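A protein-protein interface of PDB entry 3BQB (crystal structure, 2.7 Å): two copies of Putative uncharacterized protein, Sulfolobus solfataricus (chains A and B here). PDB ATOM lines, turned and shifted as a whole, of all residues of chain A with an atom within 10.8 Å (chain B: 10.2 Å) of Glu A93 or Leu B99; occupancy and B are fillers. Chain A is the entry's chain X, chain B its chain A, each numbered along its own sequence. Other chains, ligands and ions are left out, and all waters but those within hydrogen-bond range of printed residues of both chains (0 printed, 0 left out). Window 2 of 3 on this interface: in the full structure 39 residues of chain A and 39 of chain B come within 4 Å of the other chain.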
ATOM      1  N   GLU A  88       3.542  24.053  11.351  1.00  0.00           N
ATOM      2  CA  GLU A  88       3.969  23.590  12.669  1.00  0.00           C
ATOM      3  C   GLU A  88       5.489  23.679  12.748  1.00  0.00           C
ATOM      4  O   GLU A  88       6.211  23.059  11.965  1.00  0.00           O
ATOM      5  CB  GLU A  88       3.429  22.188  12.964  1.00  0.00           C
ATOM      6  CG  GLU A  88       1.918  22.210  13.251  1.00  0.00           C
ATOM      7  CD  GLU A  88       1.268  20.835  13.248  1.00  0.00           C
ATOM      8  OE1 GLU A  88       1.954  19.840  13.575  1.00  0.00           O
ATOM      9  OE2 GLU A  88       0.061  20.754  12.922  1.00  0.00           O
ATOM     10  N   ARG A  89       5.955  24.465  13.713  1.00  0.00           N
ATOM     11  CA  ARG A  89       7.267  25.101  13.635  1.00  0.00           C
ATOM     12  C   ARG A  89       8.453  24.210  13.973  1.00  0.00           C
ATOM     13  O   ARG A  89       9.600  24.635  13.827  1.00  0.00           O
ATOM     14  CB  ARG A  89       7.280  26.349  14.531  1.00  0.00           C
ATOM     15  CG  ARG A  89       6.265  27.416  14.118  1.00  0.00           C
ATOM     16  CD  ARG A  89       6.646  28.073  12.781  1.00  0.00           C
ATOM     17  NE  ARG A  89       5.567  28.886  12.212  1.00  0.00           N
ATOM     18  CZ  ARG A  89       5.665  29.597  11.087  1.00  0.00           C
ATOM     19  NH1 ARG A  89       6.798  29.611  10.387  1.00  0.00           N
ATOM     20  NH2 ARG A  89       4.623  30.303  10.661  1.00  0.00           N
ATOM     21  N   TYR A  90       8.190  22.984  14.415  1.00  0.00           N
ATOM     22  CA  TYR A  90       9.261  22.060  14.777  1.00  0.00           C
ATOM     23  C   TYR A  90       9.117  20.768  13.988  1.00  0.00           C
ATOM     24  O   TYR A  90       8.554  19.777  14.469  1.00  0.00           O
ATOM     25  CB  TYR A  90       9.282  21.840  16.295  1.00  0.00           C
ATOM     26  CG  TYR A  90       9.387  23.159  17.031  1.00  0.00           C
ATOM     27  CD1 TYR A  90      10.552  23.921  16.960  1.00  0.00           C
ATOM     28  CD2 TYR A  90       8.309  23.672  17.747  1.00  0.00           C
ATOM     29  CE1 TYR A  90      10.652  25.143  17.606  1.00  0.00           C
ATOM     30  CE2 TYR A  90       8.399  24.897  18.399  1.00  0.00           C
ATOM     31  CZ  TYR A  90       9.572  25.627  18.323  1.00  0.00           C
ATOM     32  OH  TYR A  90       9.673  26.838  18.962  1.00  0.00           O
ATOM     33  N   SER A  91       9.613  20.820  12.750  1.00  0.00           N
ATOM     34  CA  SER A  91       9.670  19.659  11.867  1.00  0.00           C
ATOM     35  C   SER A  91      10.375  18.538  12.599  1.00  0.00           C
ATOM     36  O   SER A  91      11.462  18.735  13.145  1.00  0.00           O
ATOM     37  CB  SER A  91      10.445  19.979  10.582  1.00  0.00           C
ATOM     38  OG  SER A  91       9.955  21.149   9.952  1.00  0.00           O
ATOM     39  N   GLU A  92       9.749  17.370  12.620  1.00  0.00           N
ATOM     40  CA  GLU A  92      10.353  16.201  13.228  1.00  0.00           C
ATOM     41  C   GLU A  92      11.779  16.030  12.698  1.00  0.00           C
ATOM     42  O   GLU A  92      12.045  16.227  11.511  1.00  0.00           O
ATOM     43  CB  GLU A  92       9.506  14.963  12.939  1.00  0.00           C
ATOM     44  CG  GLU A  92       9.827  13.777  13.827  1.00  0.00           C
ATOM     45  CD  GLU A  92       8.607  12.937  14.153  1.00  0.00           C
ATOM     46  OE1 GLU A  92       7.566  13.091  13.476  1.00  0.00           O
ATOM     47  OE2 GLU A  92       8.688  12.122  15.095  1.00  0.00           O
ATOM     48  N   GLU A  93      12.693  15.682  13.594  1.00  0.00           N
ATOM     49  CA  GLU A  93      14.115  15.580  13.277  1.00  0.00           C
ATOM     50  C   GLU A  93      14.387  14.248  12.575  1.00  0.00           C
ATOM     51  O   GLU A  93      15.134  13.407  13.077  1.00  0.00           O
ATOM     52  CB  GLU A  93      14.913  15.689  14.585  1.00  0.00           C
ATOM     53  CG  GLU A  93      16.430  15.804  14.453  1.00  0.00           C
ATOM     54  CD  GLU A  93      17.146  15.613  15.785  1.00  0.00           C
ATOM     55  OE1 GLU A  93      16.466  15.580  16.841  1.00  0.00           O
ATOM     56  OE2 GLU A  93      18.392  15.492  15.773  1.00  0.00           O
ATOM     57  N   ASN A  94      13.773  14.056  11.410  1.00  0.00           N
ATOM     58  CA  ASN A  94      13.807  12.757  10.731  1.00  0.00           C
ATOM     59  C   ASN A  94      13.137  12.749   9.352  1.00  0.00           C
ATOM     60  O   ASN A  94      13.543  11.989   8.471  1.00  0.00           O
ATOM     61  CB  ASN A  94      13.174  11.670  11.610  1.00  0.00           C
ATOM     62  CG  ASN A  94      13.918  10.355  11.527  1.00  0.00           C
ATOM     63  OD1 ASN A  94      14.260   9.891  10.439  1.00  0.00           O
ATOM     64  ND2 ASN A  94      14.177   9.748  12.680  1.00  0.00           N
ATOM     65  N   VAL A  95      12.101  13.567   9.170  1.00  0.00           N
ATOM     66  CA  VAL A  95      11.511  13.766   7.846  1.00  0.00           C
ATOM     67  C   VAL A  95      12.556  14.305   6.871  1.00  0.00           C
ATOM     68  O   VAL A  95      13.416  15.100   7.247  1.00  0.00           O
ATOM     69  CB  VAL A  95      10.288  14.735   7.859  1.00  0.00           C
ATOM     70  CG1 VAL A  95       9.166  14.172   8.718  1.00  0.00           C
ATOM     71  CG2 VAL A  95      10.684  16.143   8.326  1.00  0.00           C
ATOM     72  N   ALA A  96      12.476  13.860   5.621  1.00  0.00           N
ATOM     73  CA  ALA A  96      13.336  14.381   4.571  1.00  0.00           C
ATOM     74  C   ALA A  96      13.012  15.849   4.333  1.00  0.00           C
ATOM     75  O   ALA A  96      11.845  16.253   4.385  1.00  0.00           O
ATOM     76  CB  ALA A  96      13.152  13.586   3.296  1.00  0.00           C
ATOM     77  N   LYS A  97      14.048  16.646   4.082  1.00  0.00           N
ATOM     78  CA  LYS A  97      13.870  18.079   3.856  1.00  0.00           C
ATOM     79  C   LYS A  97      14.895  18.650   2.885  1.00  0.00           C
ATOM     80  O   LYS A  97      15.956  18.071   2.668  1.00  0.00           O
ATOM     81  CB  LYS A  97      13.890  18.839   5.191  1.00  0.00           C
ATOM     82  CG  LYS A  97      15.137  18.637   6.047  1.00  0.00           C
ATOM     83  CD  LYS A  97      14.784  18.353   7.514  1.00  0.00           C
ATOM     84  CE  LYS A  97      14.074  19.518   8.200  1.00  0.00           C
ATOM     85  NZ  LYS A  97      13.479  19.100   9.506  1.00  0.00           N
ATOM     86  N   ILE A  98      14.542  19.788   2.297  1.00  0.00           N
ATOM     87  CA  ILE A  98      15.340  20.428   1.263  1.00  0.00           C
ATOM     88  C   ILE A  98      15.593  21.886   1.665  1.00  0.00           C
ATOM     89  O   ILE A  98      14.653  22.686   1.749  1.00  0.00           O
ATOM     90  CB  ILE A  98      14.628  20.377  -0.118  1.00  0.00           C
ATOM     91  CG1 ILE A  98      14.149  18.956  -0.441  1.00  0.00           C
ATOM     92  CG2 ILE A  98      15.571  20.841  -1.209  1.00  0.00           C
ATOM     93  CD1 ILE A  98      13.293  18.847  -1.700  1.00  0.00           C
ATOM     94  N   LEU A  99      16.865  22.220   1.902  1.00  0.00           N
ATOM     95  CA  LEU A  99      17.259  23.518   2.468  1.00  0.00           C
ATOM     96  C   LEU A  99      16.458  23.812   3.746  1.00  0.00           C
ATOM     97  O   LEU A  99      15.935  24.918   3.929  1.00  0.00           O
ATOM     98  CB  LEU A  99      17.103  24.659   1.441  1.00  0.00           C
ATOM     99  CG  LEU A  99      18.116  24.812   0.292  1.00  0.00           C
ATOM    100  CD1 LEU A  99      19.554  24.885   0.815  1.00  0.00           C
ATOM    101  CD2 LEU A  99      17.979  23.706  -0.749  1.00  0.00           C
ATOM    102  N   GLY A 100      16.340  22.798   4.609  1.00  0.00           N
ATOM    103  CA  GLY A 100      15.679  22.945   5.910  1.00  0.00           C
ATOM    104  C   GLY A 100      14.160  22.832   5.911  1.00  0.00           C
ATOM    105  O   GLY A 100      13.568  22.459   6.927  1.00  0.00           O
ATOM    106  N   THR A 102      10.808  21.032   5.014  1.00  0.00           N
ATOM    107  CA  THR A 102      10.459  19.626   4.773  1.00  0.00           C
ATOM    108  C   THR A 102       9.761  19.439   3.418  1.00  0.00           C
ATOM    109  O   THR A 102       9.084  20.349   2.926  1.00  0.00           O
ATOM    110  CB  THR A 102       9.617  19.017   5.942  1.00  0.00           C
ATOM    111  OG1 THR A 102       9.671  17.587   5.886  1.00  0.00           O
ATOM    112  CG2 THR A 102       8.170  19.454   5.885  1.00  0.00           C
ATOM    113  N   ILE A 103       9.958  18.267   2.809  1.00  0.00           N
ATOM    114  CA  ILE A 103       9.401  17.974   1.479  1.00  0.00           C
ATOM    115  C   ILE A 103       7.888  18.163   1.447  1.00  0.00           C
ATOM    116  O   ILE A 103       7.336  18.627   0.447  1.00  0.00           O
ATOM    117  CB  ILE A 103       9.759  16.538   0.971  1.00  0.00           C
ATOM    118  CG1 ILE A 103       9.214  15.447   1.907  1.00  0.00           C
ATOM    119  CG2 ILE A 103      11.263  16.393   0.799  1.00  0.00           C
ATOM    120  CD1 ILE A 103       9.472  14.027   1.419  1.00  0.00           C
ATOM    121  N   GLU A 105       6.019  20.244   3.259  1.00  0.00           N
ATOM    122  CA  GLU A 105       5.605  21.644   3.303  1.00  0.00           C
ATOM    123  C   GLU A 105       6.164  22.450   2.127  1.00  0.00           C
ATOM    124  O   GLU A 105       5.763  23.595   1.917  1.00  0.00           O
ATOM    125  CB  GLU A 105       5.934  22.275   4.666  1.00  0.00           C
ATOM    126  CG  GLU A 105       7.362  22.778   4.860  1.00  0.00           C
ATOM    127  CD  GLU A 105       7.771  22.839   6.338  1.00  0.00           C
ATOM    128  OE1 GLU A 105       8.982  22.700   6.623  1.00  0.00           O
ATOM    129  OE2 GLU A 105       6.887  23.009   7.212  1.00  0.00           O
ATOM    130  N   ALA A 172       7.877   7.154   6.206  1.00  0.00           N
ATOM    131  CA  ALA A 172       8.703   7.918   7.142  1.00  0.00           C
ATOM    132  C   ALA A 172      10.186   7.575   6.992  1.00  0.00           C
ATOM    133  O   ALA A 172      11.023   8.473   6.935  1.00  0.00           O
ATOM    134  CB  ALA A 172       8.243   7.677   8.573  1.00  0.00           C
ATOM    135  N   GLU A 173      10.501   6.279   6.937  1.00  0.00           N
ATOM    136  CA  GLU A 173      11.875   5.814   6.705  1.00  0.00           C
ATOM    137  C   GLU A 173      12.532   6.512   5.510  1.00  0.00           C
ATOM    138  O   GLU A 173      13.686   6.950   5.593  1.00  0.00           O
ATOM    139  CB  GLU A 173      11.901   4.310   6.429  1.00  0.00           C
ATOM    140  CG  GLU A 173      11.734   3.418   7.633  1.00  0.00           C
ATOM    141  CD  GLU A 173      11.723   1.940   7.247  1.00  0.00           C
ATOM    142  OE1 GLU A 173      10.867   1.193   7.783  1.00  0.00           O
ATOM    143  OE2 GLU A 173      12.559   1.528   6.402  1.00  0.00           O
ATOM    144  N   ASN A 174      11.797   6.581   4.397  1.00  0.00           N
ATOM    145  CA  ASN A 174      12.298   7.171   3.157  1.00  0.00           C
ATOM    146  C   ASN A 174      11.135   7.508   2.221  1.00  0.00           C
ATOM    147  O   ASN A 174      10.288   6.649   1.965  1.00  0.00           O
ATOM    148  CB  ASN A 174      13.258   6.199   2.459  1.00  0.00           C
ATOM    149  CG  ASN A 174      14.284   6.909   1.598  1.00  0.00           C
ATOM    150  OD1 ASN A 174      13.950   7.796   0.816  1.00  0.00           O
ATOM    151  ND2 ASN A 174      15.548   6.524   1.745  1.00  0.00           N
ATOM    152  N   PRO A 175      11.080   8.752   1.709  1.00  0.00           N
ATOM    153  CA  PRO A 175      10.031   9.035   0.723  1.00  0.00           C
ATOM    154  C   PRO A 175      10.093   8.150  -0.533  1.00  0.00           C
ATOM    155  O   PRO A 175       9.089   8.023  -1.232  1.00  0.00           O
ATOM    156  CB  PRO A 175      10.244  10.516   0.371  1.00  0.00           C
ATOM    157  CG  PRO A 175      11.608  10.851   0.849  1.00  0.00           C
ATOM    158  CD  PRO A 175      11.901   9.941   1.998  1.00  0.00           C
ATOM    159  N   VAL B  95      19.497  18.564  -3.371  1.00  0.00           N
ATOM    160  CA  VAL B  95      18.608  17.418  -3.115  1.00  0.00           C
ATOM    161  C   VAL B  95      18.102  17.295  -1.670  1.00  0.00           C
ATOM    162  O   VAL B  95      18.617  17.944  -0.758  1.00  0.00           O
ATOM    163  CB  VAL B  95      19.275  16.068  -3.518  1.00  0.00           C
ATOM    164  CG1 VAL B  95      19.557  16.035  -5.019  1.00  0.00           C
ATOM    165  CG2 VAL B  95      20.550  15.807  -2.707  1.00  0.00           C
ATOM    166  N   ALA B  96      17.087  16.446  -1.490  1.00  0.00           N
ATOM    167  CA  ALA B  96      16.485  16.171  -0.184  1.00  0.00           C
ATOM    168  C   ALA B  96      17.331  15.196   0.625  1.00  0.00           C
ATOM    169  O   ALA B  96      18.054  14.366   0.064  1.00  0.00           O
ATOM    170  CB  ALA B  96      15.077  15.620  -0.360  1.00  0.00           C
ATOM    171  N   LYS B  97      17.219  15.288   1.948  1.00  0.00           N
ATOM    172  CA  LYS B  97      18.097  14.535   2.846  1.00  0.00           C
ATOM    173  C   LYS B  97      17.488  14.294   4.228  1.00  0.00           C
ATOM    174  O   LYS B  97      16.762  15.138   4.755  1.00  0.00           O
ATOM    175  CB  LYS B  97      19.468  15.228   2.959  1.00  0.00           C
ATOM    176  CG  LYS B  97      19.432  16.760   3.016  1.00  0.00           C
ATOM    177  CD  LYS B  97      20.417  17.395   2.023  1.00  0.00           C
ATOM    178  CE  LYS B  97      21.871  17.088   2.361  1.00  0.00           C
ATOM    179  NZ  LYS B  97      22.809  17.846   1.487  1.00  0.00           N
ATOM    180  N   ILE B  98      17.793  13.122   4.784  1.00  0.00           N
ATOM    181  CA  ILE B  98      17.334  12.702   6.107  1.00  0.00           C
ATOM    182  C   ILE B  98      18.524  12.697   7.075  1.00  0.00           C
ATOM    183  O   ILE B  98      19.413  11.843   6.976  1.00  0.00           O
ATOM    184  CB  ILE B  98      16.692  11.285   6.056  1.00  0.00           C
ATOM    185  CG1 ILE B  98      15.434  11.295   5.178  1.00  0.00           C
ATOM    186  CG2 ILE B  98      16.355  10.784   7.468  1.00  0.00           C
ATOM    187  CD1 ILE B  98      14.903   9.919   4.838  1.00  0.00           C
ATOM    188  N   LEU B  99      18.515  13.647   8.011  1.00  0.00           N
ATOM    189  CA  LEU B  99      19.597  13.834   8.979  1.00  0.00           C
ATOM    190  C   LEU B  99      20.914  14.102   8.254  1.00  0.00           C
ATOM    191  O   LEU B  99      21.874  13.342   8.394  1.00  0.00           O
ATOM    192  CB  LEU B  99      19.735  12.616   9.911  1.00  0.00           C
ATOM    193  CG  LEU B  99      18.534  12.230  10.778  1.00  0.00           C
ATOM    194  CD1 LEU B  99      18.724  10.827  11.346  1.00  0.00           C
ATOM    195  CD2 LEU B  99      18.311  13.246  11.893  1.00  0.00           C
ATOM    196  N   GLY B 100      20.945  15.164   7.446  1.00  0.00           N
ATOM    197  CA  GLY B 100      22.142  15.524   6.676  1.00  0.00           C
ATOM    198  C   GLY B 100      22.452  14.591   5.509  1.00  0.00           C
ATOM    199  O   GLY B 100      22.899  15.043   4.453  1.00  0.00           O
ATOM    200  N   LYS B 101      22.224  13.290   5.711  1.00  0.00           N
ATOM    201  CA  LYS B 101      22.472  12.252   4.708  1.00  0.00           C
ATOM    202  C   LYS B 101      21.380  12.274   3.633  1.00  0.00           C
ATOM    203  O   LYS B 101      20.200  12.396   3.954  1.00  0.00           O
ATOM    204  CB  LYS B 101      22.506  10.887   5.403  1.00  0.00           C
ATOM    205  CG  LYS B 101      23.095   9.757   4.589  1.00  0.00           C
ATOM    206  CD  LYS B 101      23.243   8.507   5.449  1.00  0.00           C
ATOM    207  CE  LYS B 101      23.629   7.296   4.620  1.00  0.00           C
ATOM    208  NZ  LYS B 101      23.785   6.079   5.458  1.00  0.00           N
ATOM    209  N   THR B 102      21.777  12.153   2.365  1.00  0.00           N
ATOM    210  CA  THR B 102      20.845  12.274   1.233  1.00  0.00           C
ATOM    211  C   THR B 102      19.945  11.029   1.113  1.00  0.00           C
ATOM    212  O   THR B 102      20.366   9.915   1.453  1.00  0.00           O
ATOM    213  CB  THR B 102      21.606  12.594  -0.104  1.00  0.00           C
ATOM    214  OG1 THR B 102      20.773  13.381  -0.960  1.00  0.00           O
ATOM    215  CG2 THR B 102      22.046  11.341  -0.848  1.00  0.00           C
ATOM    216  N   ILE B 103      18.707  11.228   0.649  1.00  0.00           N
ATOM    217  CA  ILE B 103      17.706  10.141   0.603  1.00  0.00           C
ATOM    218  C   ILE B 103      18.123   8.981  -0.305  1.00  0.00           C
ATOM    219  O   ILE B 103      17.748   7.835  -0.068  1.00  0.00           O
ATOM    220  CB  ILE B 103      16.287  10.642   0.177  1.00  0.00           C
ATOM    221  CG1 ILE B 103      16.277  11.153  -1.266  1.00  0.00           C
ATOM    222  CG2 ILE B 103      15.788  11.729   1.122  1.00  0.00           C
ATOM    223  CD1 ILE B 103      14.911  11.601  -1.740  1.00  0.00           C
ATOM    224  N   GLU B 105      21.354   7.840  -0.991  1.00  0.00           N
ATOM    225  CA  GLU B 105      22.364   6.970  -0.388  1.00  0.00           C
ATOM    226  C   GLU B 105      21.837   6.244   0.854  1.00  0.00           C
ATOM    227  O   GLU B 105      22.393   5.220   1.251  1.00  0.00           O
ATOM    228  CB  GLU B 105      23.649   7.741  -0.082  1.00  0.00           C
ATOM    229  CG  GLU B 105      23.594   8.668   1.117  1.00  0.00           C
ATOM    230  CD  GLU B 105      24.672   9.746   1.061  1.00  0.00           C
ATOM    231  OE1 GLU B 105      24.422  10.877   1.542  1.00  0.00           O
ATOM    232  OE2 GLU B 105      25.769   9.460   0.524  1.00  0.00           O
ATOM    233  N   LYS B 106      20.771   6.766   1.460  1.00  0.00           N
ATOM    234  CA  LYS B 106      20.039   6.013   2.488  1.00  0.00           C
ATOM    235  C   LYS B 106      19.462   4.734   1.894  1.00  0.00           C
ATOM    236  O   LYS B 106      19.570   3.669   2.500  1.00  0.00           O
ATOM    237  CB  LYS B 106      18.906   6.839   3.118  1.00  0.00           C
ATOM    238  CG  LYS B 106      19.341   7.735   4.270  1.00  0.00           C
ATOM    239  CD  LYS B 106      18.553   7.449   5.553  1.00  0.00           C
ATOM    240  CE  LYS B 106      19.165   8.185   6.749  1.00  0.00           C
ATOM    241  NZ  LYS B 106      18.868   7.518   8.046  1.00  0.00           N
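The side-chain hydroxyl (OG1) of Thr B102 lies within hydrogen-bond range of the backbone carbonyl oxygen (O) of Ala B96, at 3.1 Å.
The backbone carbonyl oxygen of Ala B96 sits at hydrogen-bond distance from the backbone NH of Ile B103 (3.3 Å).
OG1 of Thr A102 sits at hydrogen-bond distance from O of Ala A96, at 3.0 Å.
The backbone NH (N) of Ile A103 is in hydrogen-bond range of the backbone carbonyl oxygen (O) of Ala A96 (3.2 Å).
Among the printed residues, merely in contact across the chains: Glu A93 with Leu B99 (3.4 Å), Asn A94 with Ile B98 (3.2 Å), Ala A96 with Lys B97 (3.5 Å), Ala A96 with Ile B98 (3.7 Å), Ala A96 with Ile B103 (3.9 Å), Lys A97 with Ala B96 (3.5 Å), Ile A98 with Ala B96 (3.5 Å), Glu A173 with Ile B98 (3.3 Å) and Asn A174 with Lys B106 (3.6 Å).
The backbone NH (N) of Lys B97 is in hydrogen-bond range of the backbone carbonyl oxygen (O) of Lys A97 (3.1 Å).
O of Ile B103 lies within hydrogen-bond range of ND2 of Asn A174 (3.1 Å).
Of chain B, only Leu B99 (3.4 Å) comes within 4 Å of Glu A93.
Of chain A, only Glu A93 comes within 4 Å of Leu B99.
No residue of chain B comes within 4 Å of Glu A92.
Of chain B, only Ile B98 comes within 4 Å of Asn A94.
Ile B98 touches just these residues of chain A: Asn A94, Ala A96 and Glu A173.
No residue of chain A comes within 4 Å of Gly B100.
Printed residues of chain B within 4 Å of Ile A98: Ala B96 (3.5 Å).
Printed residues of chain B within 4 Å of Asn A174: Ile B103 (3.1 Å) and Lys B106 (3.6 Å).
Printed residues of chain B within 4 Å of Glu A173: Ile B98 (3.3 Å).
Printed residues of chain A within 4 Å of Ala B96: Lys A97 and Ile A98.
Arg A89 touches none of the printed residues of chain B.
Val B95 touches none of the printed residues of chain A.
The nearest residue of chain B that does not touch Glu A93 is Ile B98 (6.3 Å).
The nearest residue of chain A that does not touch Leu B99 is Asn A94 (4.6 Å).
The nearest printed residue of chain B that does not touch Ala A96 is Ala B96 (4.6 Å).
Of the 11 printed residues of chain B, 6 touch a printed residue of chain A.
Of the 20 printed residues of chain A, 7 touch a printed residue of chain B.
Hydrophobic or aromatic side chains of chain A that line the printed part of chain B: Ala A96 and Ile A98.
Among the printed residues, no Asp or Glu carboxylate lies within 4 Å of a Lys or Arg side-chain nitrogen of the other chain.
Ala A96 touches Lys B97, and with the chains exchanged Lys A97 touches Ala B96.
Ala A96 touches Ile B98, and with the chains exchanged Ile A98 touches Ala B96.
Ala A96 touches Ile B103, but with the chains exchanged Ile A103 does not touch Ala B96 (4.1 Å).
Lys A97 touches its own counterpart, Lys B97.
Positions printed for both chains: 95, 96, 97, 98, 99, 100, 102, 103 and 105.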
